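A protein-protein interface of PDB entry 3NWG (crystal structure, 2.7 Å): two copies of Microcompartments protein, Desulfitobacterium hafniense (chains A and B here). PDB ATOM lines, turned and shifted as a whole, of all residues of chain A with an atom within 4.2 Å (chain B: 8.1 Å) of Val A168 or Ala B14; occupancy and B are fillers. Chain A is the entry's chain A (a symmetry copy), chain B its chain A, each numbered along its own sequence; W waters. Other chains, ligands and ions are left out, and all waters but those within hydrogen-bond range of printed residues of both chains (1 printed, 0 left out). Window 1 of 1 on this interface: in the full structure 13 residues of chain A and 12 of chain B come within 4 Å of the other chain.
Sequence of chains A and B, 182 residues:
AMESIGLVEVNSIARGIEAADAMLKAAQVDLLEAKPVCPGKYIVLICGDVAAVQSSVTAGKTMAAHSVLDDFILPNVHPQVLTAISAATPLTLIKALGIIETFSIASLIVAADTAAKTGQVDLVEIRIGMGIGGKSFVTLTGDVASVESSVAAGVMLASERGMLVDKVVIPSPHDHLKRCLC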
ATOM      1  N   LEU A  97       1.847  -4.399 -12.217  1.00  0.00           N
ATOM      2  CA  LEU A  97       0.477  -4.887 -12.233  1.00  0.00           C
ATOM      3  C   LEU A  97      -0.015  -5.327 -10.858  1.00  0.00           C
ATOM      4  O   LEU A  97       0.520  -6.256 -10.256  1.00  0.00           O
ATOM      5  CB  LEU A  97       0.343  -6.033 -13.233  1.00  0.00           C
ATOM      6  CG  LEU A  97      -1.039  -6.658 -13.437  1.00  0.00           C
ATOM      7  CD1 LEU A  97      -1.951  -5.761 -14.273  1.00  0.00           C
ATOM      8  CD2 LEU A  97      -0.897  -8.002 -14.107  1.00  0.00           C
ATOM      9  N   GLY A  98      -1.047  -4.645 -10.377  1.00  0.00           N
ATOM     10  CA  GLY A  98      -1.688  -4.986  -9.122  1.00  0.00           C
ATOM     11  C   GLY A  98      -3.051  -5.616  -9.342  1.00  0.00           C
ATOM     12  O   GLY A  98      -3.770  -5.256 -10.268  1.00  0.00           O
ATOM     13  N   ILE A  99      -3.389  -6.583  -8.496  1.00  0.00           N
ATOM     14  CA  ILE A  99      -4.678  -7.265  -8.561  1.00  0.00           C
ATOM     15  C   ILE A  99      -5.216  -7.437  -7.148  1.00  0.00           C
ATOM     16  O   ILE A  99      -4.500  -7.944  -6.270  1.00  0.00           O
ATOM     17  CB  ILE A  99      -4.576  -8.670  -9.211  1.00  0.00           C
ATOM     18  CG1 ILE A  99      -3.796  -8.622 -10.536  1.00  0.00           C
ATOM     19  CG2 ILE A  99      -5.967  -9.258  -9.403  1.00  0.00           C
ATOM     20  CD1 ILE A  99      -3.373 -10.024 -11.101  1.00  0.00           C
ATOM     21  N   GLU A 101      -8.572  -9.157  -5.094  1.00  0.00           N
ATOM     22  CA  GLU A 101      -9.629 -10.126  -5.305  1.00  0.00           C
ATOM     23  C   GLU A 101     -10.368 -10.339  -3.984  1.00  0.00           C
ATOM     24  O   GLU A 101      -9.750 -10.676  -2.976  1.00  0.00           O
ATOM     25  CB  GLU A 101      -9.022 -11.419  -5.848  1.00  0.00           C
ATOM     26  CG  GLU A 101      -9.964 -12.582  -6.135  1.00  0.00           C
ATOM     27  CD  GLU A 101      -9.192 -13.915  -6.274  1.00  0.00           C
ATOM     28  OE1 GLU A 101      -7.967 -13.931  -6.016  1.00  0.00           O
ATOM     29  OE2 GLU A 101      -9.784 -14.952  -6.634  1.00  0.00           O
ATOM     30  N   LYS A 167      -4.287 -10.604  -2.914  1.00  0.00           N
ATOM     31  CA  LYS A 167      -3.749  -9.574  -3.801  1.00  0.00           C
ATOM     32  C   LYS A 167      -2.316  -9.895  -4.207  1.00  0.00           C
ATOM     33  O   LYS A 167      -1.632 -10.670  -3.544  1.00  0.00           O
ATOM     34  CB  LYS A 167      -3.783  -8.181  -3.160  1.00  0.00           C
ATOM     35  CG  LYS A 167      -3.703  -8.131  -1.637  1.00  0.00           C
ATOM     36  CD  LYS A 167      -2.378  -8.494  -1.036  1.00  0.00           C
ATOM     37  CE  LYS A 167      -2.608  -8.883   0.421  1.00  0.00           C
ATOM     38  NZ  LYS A 167      -1.392  -9.469   1.023  1.00  0.00           N
ATOM     39  N   VAL A 168      -1.882  -9.300  -5.311  1.00  0.00           N
ATOM     40  CA  VAL A 168      -0.528  -9.459  -5.796  1.00  0.00           C
ATOM     41  C   VAL A 168      -0.102  -8.150  -6.434  1.00  0.00           C
ATOM     42  O   VAL A 168      -0.936  -7.431  -6.996  1.00  0.00           O
ATOM     43  CB  VAL A 168      -0.381 -10.643  -6.817  1.00  0.00           C
ATOM     44  CG1 VAL A 168      -0.838 -11.954  -6.206  1.00  0.00           C
ATOM     45  CG2 VAL A 168      -1.106 -10.369  -8.122  1.00  0.00           C
ATOM     46  N   VAL A 169       1.182  -7.833  -6.309  1.00  0.00           N
ATOM     47  CA  VAL A 169       1.821  -6.819  -7.142  1.00  0.00           C
ATOM     48  C   VAL A 169       2.908  -7.526  -7.954  1.00  0.00           C
ATOM     49  O   VAL A 169       3.795  -8.186  -7.399  1.00  0.00           O
ATOM     50  CB  VAL A 169       2.387  -5.643  -6.306  1.00  0.00           C
ATOM     51  CG1 VAL A 169       3.197  -4.679  -7.172  1.00  0.00           C
ATOM     52  CG2 VAL A 169       1.260  -4.894  -5.571  1.00  0.00           C
ATOM     53  N   ILE A 170       2.796  -7.424  -9.270  1.00  0.00           N
ATOM     54  CA  ILE A 170       3.749  -8.016 -10.172  1.00  0.00           C
ATOM     55  C   ILE A 170       4.440  -6.851 -10.855  1.00  0.00           C
ATOM     56  O   ILE A 170       3.840  -6.216 -11.716  1.00  0.00           O
ATOM     57  CB  ILE A 170       3.037  -8.926 -11.204  1.00  0.00           C
ATOM     58  CG1 ILE A 170       2.158  -9.957 -10.481  1.00  0.00           C
ATOM     59  CG2 ILE A 170       4.042  -9.599 -12.176  1.00  0.00           C
ATOM     60  CD1 ILE A 170       1.192 -10.718 -11.400  1.00  0.00           C
ATOM     61  N   VAL B  10      -4.332 -23.234  -8.497  1.00  0.00           N
ATOM     62  CA  VAL B  10      -4.214 -22.221  -7.452  1.00  0.00           C
ATOM     63  C   VAL B  10      -5.596 -21.750  -7.019  1.00  0.00           C
ATOM     64  O   VAL B  10      -6.509 -21.646  -7.831  1.00  0.00           O
ATOM     65  CB  VAL B  10      -3.412 -20.978  -7.939  1.00  0.00           C
ATOM     66  CG1 VAL B  10      -3.205 -19.992  -6.820  1.00  0.00           C
ATOM     67  CG2 VAL B  10      -2.055 -21.381  -8.510  1.00  0.00           C
ATOM     68  N   ASN B  11      -5.735 -21.461  -5.736  1.00  0.00           N
ATOM     69  CA  ASN B  11      -6.957 -20.968  -5.134  1.00  0.00           C
ATOM     70  C   ASN B  11      -7.434 -19.559  -5.537  1.00  0.00           C
ATOM     71  O   ASN B  11      -8.609 -19.256  -5.404  1.00  0.00           O
ATOM     72  CB  ASN B  11      -6.749 -20.982  -3.632  1.00  0.00           C
ATOM     73  CG  ASN B  11      -8.001 -21.317  -2.885  1.00  0.00           C
ATOM     74  OD1 ASN B  11      -8.988 -21.818  -3.460  1.00  0.00           O
ATOM     75  ND2 ASN B  11      -7.985 -21.047  -1.578  1.00  0.00           N
ATOM     76  N   SER B  12      -6.536 -18.687  -5.977  1.00  0.00           N
ATOM     77  CA  SER B  12      -6.901 -17.331  -6.391  1.00  0.00           C
ATOM     78  C   SER B  12      -6.575 -17.063  -7.832  1.00  0.00           C
ATOM     79  O   SER B  12      -5.536 -17.498  -8.333  1.00  0.00           O
ATOM     80  CB  SER B  12      -6.090 -16.293  -5.629  1.00  0.00           C
ATOM     81  OG  SER B  12      -6.368 -16.359  -4.273  1.00  0.00           O
ATOM     82  N   ILE B  13      -7.416 -16.269  -8.479  1.00  0.00           N
ATOM     83  CA  ILE B  13      -7.007 -15.626  -9.719  1.00  0.00           C
ATOM     84  C   ILE B  13      -5.704 -14.822  -9.491  1.00  0.00           C
ATOM     85  O   ILE B  13      -4.697 -15.051 -10.177  1.00  0.00           O
ATOM     86  CB  ILE B  13      -8.138 -14.747 -10.301  1.00  0.00           C
ATOM     87  CG1 ILE B  13      -9.260 -15.640 -10.866  1.00  0.00           C
ATOM     88  CG2 ILE B  13      -7.595 -13.845 -11.404  1.00  0.00           C
ATOM     89  CD1 ILE B  13     -10.357 -16.045  -9.871  1.00  0.00           C
ATOM     90  N   ALA B  14      -5.722 -13.926  -8.501  1.00  0.00           N
ATOM     91  CA  ALA B  14      -4.573 -13.053  -8.226  1.00  0.00           C
ATOM     92  C   ALA B  14      -3.268 -13.852  -8.132  1.00  0.00           C
ATOM     93  O   ALA B  14      -2.335 -13.628  -8.915  1.00  0.00           O
ATOM     94  CB  ALA B  14      -4.806 -12.225  -6.976  1.00  0.00           C
ATOM     95  N   ARG B  15      -3.238 -14.808  -7.207  1.00  0.00           N
ATOM     96  CA  ARG B  15      -2.103 -15.719  -7.024  1.00  0.00           C
ATOM     97  C   ARG B  15      -1.798 -16.575  -8.238  1.00  0.00           C
ATOM     98  O   ARG B  15      -0.635 -16.853  -8.516  1.00  0.00           O
ATOM     99  CB  ARG B  15      -2.345 -16.637  -5.826  1.00  0.00           C
ATOM    100  CG  ARG B  15      -2.354 -15.916  -4.490  1.00  0.00           C
ATOM    101  CD  ARG B  15      -0.975 -15.385  -4.117  1.00  0.00           C
ATOM    102  NE  ARG B  15      -0.718 -15.642  -2.697  1.00  0.00           N
ATOM    103  CZ  ARG B  15       0.238 -16.448  -2.243  1.00  0.00           C
ATOM    104  NH1 ARG B  15       0.388 -16.641  -0.949  1.00  0.00           N
ATOM    105  NH2 ARG B  15       1.056 -17.050  -3.085  1.00  0.00           N
ATOM    106  N   GLY B  16      -2.843 -16.996  -8.950  1.00  0.00           N
ATOM    107  CA  GLY B  16      -2.695 -17.804 -10.147  1.00  0.00           C
ATOM    108  C   GLY B  16      -1.997 -17.012 -11.232  1.00  0.00           C
ATOM    109  O   GLY B  16      -1.159 -17.547 -11.968  1.00  0.00           O
ATOM    110  N   ILE B  17      -2.336 -15.731 -11.342  1.00  0.00           N
ATOM    111  CA  ILE B  17      -1.702 -14.872 -12.325  1.00  0.00           C
ATOM    112  C   ILE B  17      -0.229 -14.617 -11.960  1.00  0.00           C
ATOM    113  O   ILE B  17       0.621 -14.545 -12.844  1.00  0.00           O
ATOM    114  CB  ILE B  17      -2.495 -13.582 -12.519  1.00  0.00           C
ATOM    115  CG1 ILE B  17      -3.806 -13.909 -13.262  1.00  0.00           C
ATOM    116  CG2 ILE B  17      -1.683 -12.540 -13.268  1.00  0.00           C
ATOM    117  CD1 ILE B  17      -4.847 -12.770 -13.268  1.00  0.00           C
ATOM    118  N   GLU B  18       0.066 -14.516 -10.664  1.00  0.00           N
ATOM    119  CA  GLU B  18       1.427 -14.308 -10.203  1.00  0.00           C
ATOM    120  C   GLU B  18       2.207 -15.595 -10.382  1.00  0.00           C
ATOM    121  O   GLU B  18       3.394 -15.571 -10.734  1.00  0.00           O
ATOM    122  CB  GLU B  18       1.453 -13.893  -8.731  1.00  0.00           C
ATOM    123  CG  GLU B  18       2.827 -13.474  -8.212  1.00  0.00           C
ATOM    124  CD  GLU B  18       2.848 -13.237  -6.691  1.00  0.00           C
ATOM    125  OE1 GLU B  18       2.351 -14.091  -5.922  1.00  0.00           O
ATOM    126  OE2 GLU B  18       3.378 -12.190  -6.243  1.00  0.00           O
ATOM    127  N   ALA B  19       1.543 -16.722 -10.138  1.00  0.00           N
ATOM    128  CA  ALA B  19       2.203 -18.002 -10.291  1.00  0.00           C
ATOM    129  C   ALA B  19       2.558 -18.198 -11.759  1.00  0.00           C
ATOM    130  O   ALA B  19       3.651 -18.669 -12.075  1.00  0.00           O
ATOM    131  CB  ALA B  19       1.326 -19.131  -9.779  1.00  0.00           C
ATOM    132  N   ALA B  20       1.645 -17.810 -12.653  1.00  0.00           N
ATOM    133  CA  ALA B  20       1.840 -18.004 -14.092  1.00  0.00           C
ATOM    134  C   ALA B  20       3.021 -17.180 -14.565  1.00  0.00           C
ATOM    135  O   ALA B  20       3.794 -17.620 -15.410  1.00  0.00           O
ATOM    136  CB  ALA B  20       0.584 -17.638 -14.875  1.00  0.00           C
ATOM    137  N   ASP B  21       3.173 -15.998 -13.985  1.00  0.00           N
ATOM    138  CA  ASP B  21       4.262 -15.101 -14.327  1.00  0.00           C
ATOM    139  C   ASP B  21       5.605 -15.713 -13.954  1.00  0.00           C
ATOM    140  O   ASP B  21       6.549 -15.645 -14.731  1.00  0.00           O
ATOM    141  CB  ASP B  21       4.092 -13.775 -13.590  1.00  0.00           C
ATOM    142  CG  ASP B  21       5.093 -12.726 -14.037  1.00  0.00           C
ATOM    143  OD1 ASP B  21       4.927 -12.224 -15.170  1.00  0.00           O
ATOM    144  OD2 ASP B  21       6.039 -12.399 -13.268  1.00  0.00           O
ATOM    145  N   GLY B  40     -12.786 -21.395  -6.821  1.00  0.00           N
ATOM    146  CA  GLY B  40     -12.540 -20.196  -7.625  1.00  0.00           C
ATOM    147  C   GLY B  40     -11.187 -20.372  -8.293  1.00  0.00           C
ATOM    148  O   GLY B  40     -10.497 -19.386  -8.606  1.00  0.00           O
ATOM    149  N   TYR B  42      -7.717 -21.214 -10.306  1.00  0.00           N
ATOM    150  CA  TYR B  42      -7.016 -20.764 -11.481  1.00  0.00           C
ATOM    151  C   TYR B  42      -6.046 -21.876 -11.830  1.00  0.00           C
ATOM    152  O   TYR B  42      -5.401 -22.455 -10.948  1.00  0.00           O
ATOM    153  CB  TYR B  42      -6.253 -19.492 -11.177  1.00  0.00           C
ATOM    154  CG  TYR B  42      -5.799 -18.749 -12.411  1.00  0.00           C
ATOM    155  CD1 TYR B  42      -6.648 -17.853 -13.050  1.00  0.00           C
ATOM    156  CD2 TYR B  42      -4.515 -18.932 -12.935  1.00  0.00           C
ATOM    157  CE1 TYR B  42      -6.244 -17.164 -14.171  1.00  0.00           C
ATOM    158  CE2 TYR B  42      -4.100 -18.243 -14.056  1.00  0.00           C
ATOM    159  CZ  TYR B  42      -4.975 -17.359 -14.672  1.00  0.00           C
ATOM    160  OH  TYR B  42      -4.589 -16.658 -15.791  1.00  0.00           O
ATOM    161  N   MET B  63       5.707 -19.180  -5.721  1.00  0.00           N
ATOM    162  CA  MET B  63       4.929 -17.954  -5.630  1.00  0.00           C
ATOM    163  C   MET B  63       3.583 -18.195  -4.990  1.00  0.00           C
ATOM    164  O   MET B  63       3.200 -17.466  -4.083  1.00  0.00           O
ATOM    165  CB  MET B  63       4.754 -17.275  -6.986  1.00  0.00           C
ATOM    166  CG  MET B  63       6.067 -16.802  -7.618  1.00  0.00           C
ATOM    167  SD  MET B  63       7.162 -15.614  -6.522  1.00  0.00           S
ATOM    168  CE  MET B  63       5.805 -14.338  -6.072  1.00  0.00           C
ATOM    169  N   ALA B  64       2.886 -19.233  -5.437  1.00  0.00           N
ATOM    170  CA  ALA B  64       1.553 -19.533  -4.934  1.00  0.00           C
ATOM    171  C   ALA B  64       1.486 -20.115  -3.501  1.00  0.00           C
ATOM    172  O   ALA B  64       0.486 -19.944  -2.818  1.00  0.00           O
ATOM    173  CB  ALA B  64       0.801 -20.401  -5.926  1.00  0.00           C
ATOM    174  N   SER B  67      -1.849 -21.401  -1.388  1.00  0.00           N
ATOM    175  CA  SER B  67      -3.030 -21.388  -2.228  1.00  0.00           C
ATOM    176  C   SER B  67      -2.877 -22.345  -3.413  1.00  0.00           C
ATOM    177  O   SER B  67      -3.692 -22.333  -4.341  1.00  0.00           O
ATOM    178  CB  SER B  67      -3.379 -19.964  -2.673  1.00  0.00           C
ATOM    179  OG  SER B  67      -2.401 -19.439  -3.536  1.00  0.00           O
HETATM  180  O   HOH W   1       5.043 -10.685  -7.647  1.00  0.00           O
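The side-chain carboxylate (OE1) of Glu A101 lies close to the side-chain hydroxyl (OG) of Ser B12. The backbone NH of Ala B14 lies within hydrogen-bond range of the side-chain carboxylate of Glu A101 (3.3 Å). OE2 of Glu A101 is in hydrogen-bond range of N of Ile B13, 3.3 Å away.
O of Met B63 is in hydrogen-bond range of NH2 of Arg B15 (2.4 Å). The guanidinium group (NH2) of Arg B15 is in hydrogen-bond range of the backbone carbonyl oxygen (O) of Ala B64 (3.0 Å). The backbone NH of Ile A170 lies within hydrogen-bond range of the backbone carbonyl oxygen of Leu A97, at 2.7 Å. The backbone NH (N) of Ile A99 lies within hydrogen-bond range of the backbone carbonyl oxygen (O) of Val A168, at 3.0 Å.
Among the printed residues, pairs that only touch across the chains: Val A168 with Ala B14 (3.5 Å), Ile A170 with Asp B21 (3.6 Å), Ile A99 with Ile B17 (3.7 Å), Ile A170 with Glu B18 (3.8 Å), Val A168 with Glu B18 (3.8 Å), Val A168 with Arg B15 (3.9 Å) and Ile A170 with Ile B17 (3.9 Å).
Of chain B, only Ala B14 (3.5 Å), Arg B15 (3.9 Å) and Glu B18 (3.8 Å) come within 4 Å of Val A168. Of the printed residues of chain A, Ala B14 touches Glu A101 and Val A168. Of the printed residues of chain A, Arg B15 touches Val A168 (3.9 Å). Of the printed residues of chain A, Ile B17 touches Ile A99 and Ile A170. Printed residues of chain A within 4 Å of Glu B18: Val A168 and Ile A170. Of the printed residues of chain A, Asp B21 touches Ile A170 (3.6 Å). The nearest residue of chain B that does not touch Val A168 is Ile B17 (5.6 Å). The nearest printed residue of chain A that does not touch Ile B17 is Leu A97 (4.7 Å).
Of the 17 printed residues of chain B, 7 touch a printed residue of chain A. Hydrophobic or aromatic side chains of chain B within 4 Å of the printed part of chain A: Ile B13, Ala B14 and Ile B17. Of the 8 printed residues of chain A, 4 touch a printed residue of chain B. Printed residues of chain A that touch a printed residue of chain B: Ile A99, Glu A101, Val A168 and Ile A170.
No position is printed for both chains. Of the 10 pairs that touch across the chains among the printed residues, none has its exchanged pair printed and touching as well.
Water W1 lies within hydrogen-bond range of OE2 of Glu B18 (2.6 Å) and O of Val A169 (2.8 Å).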
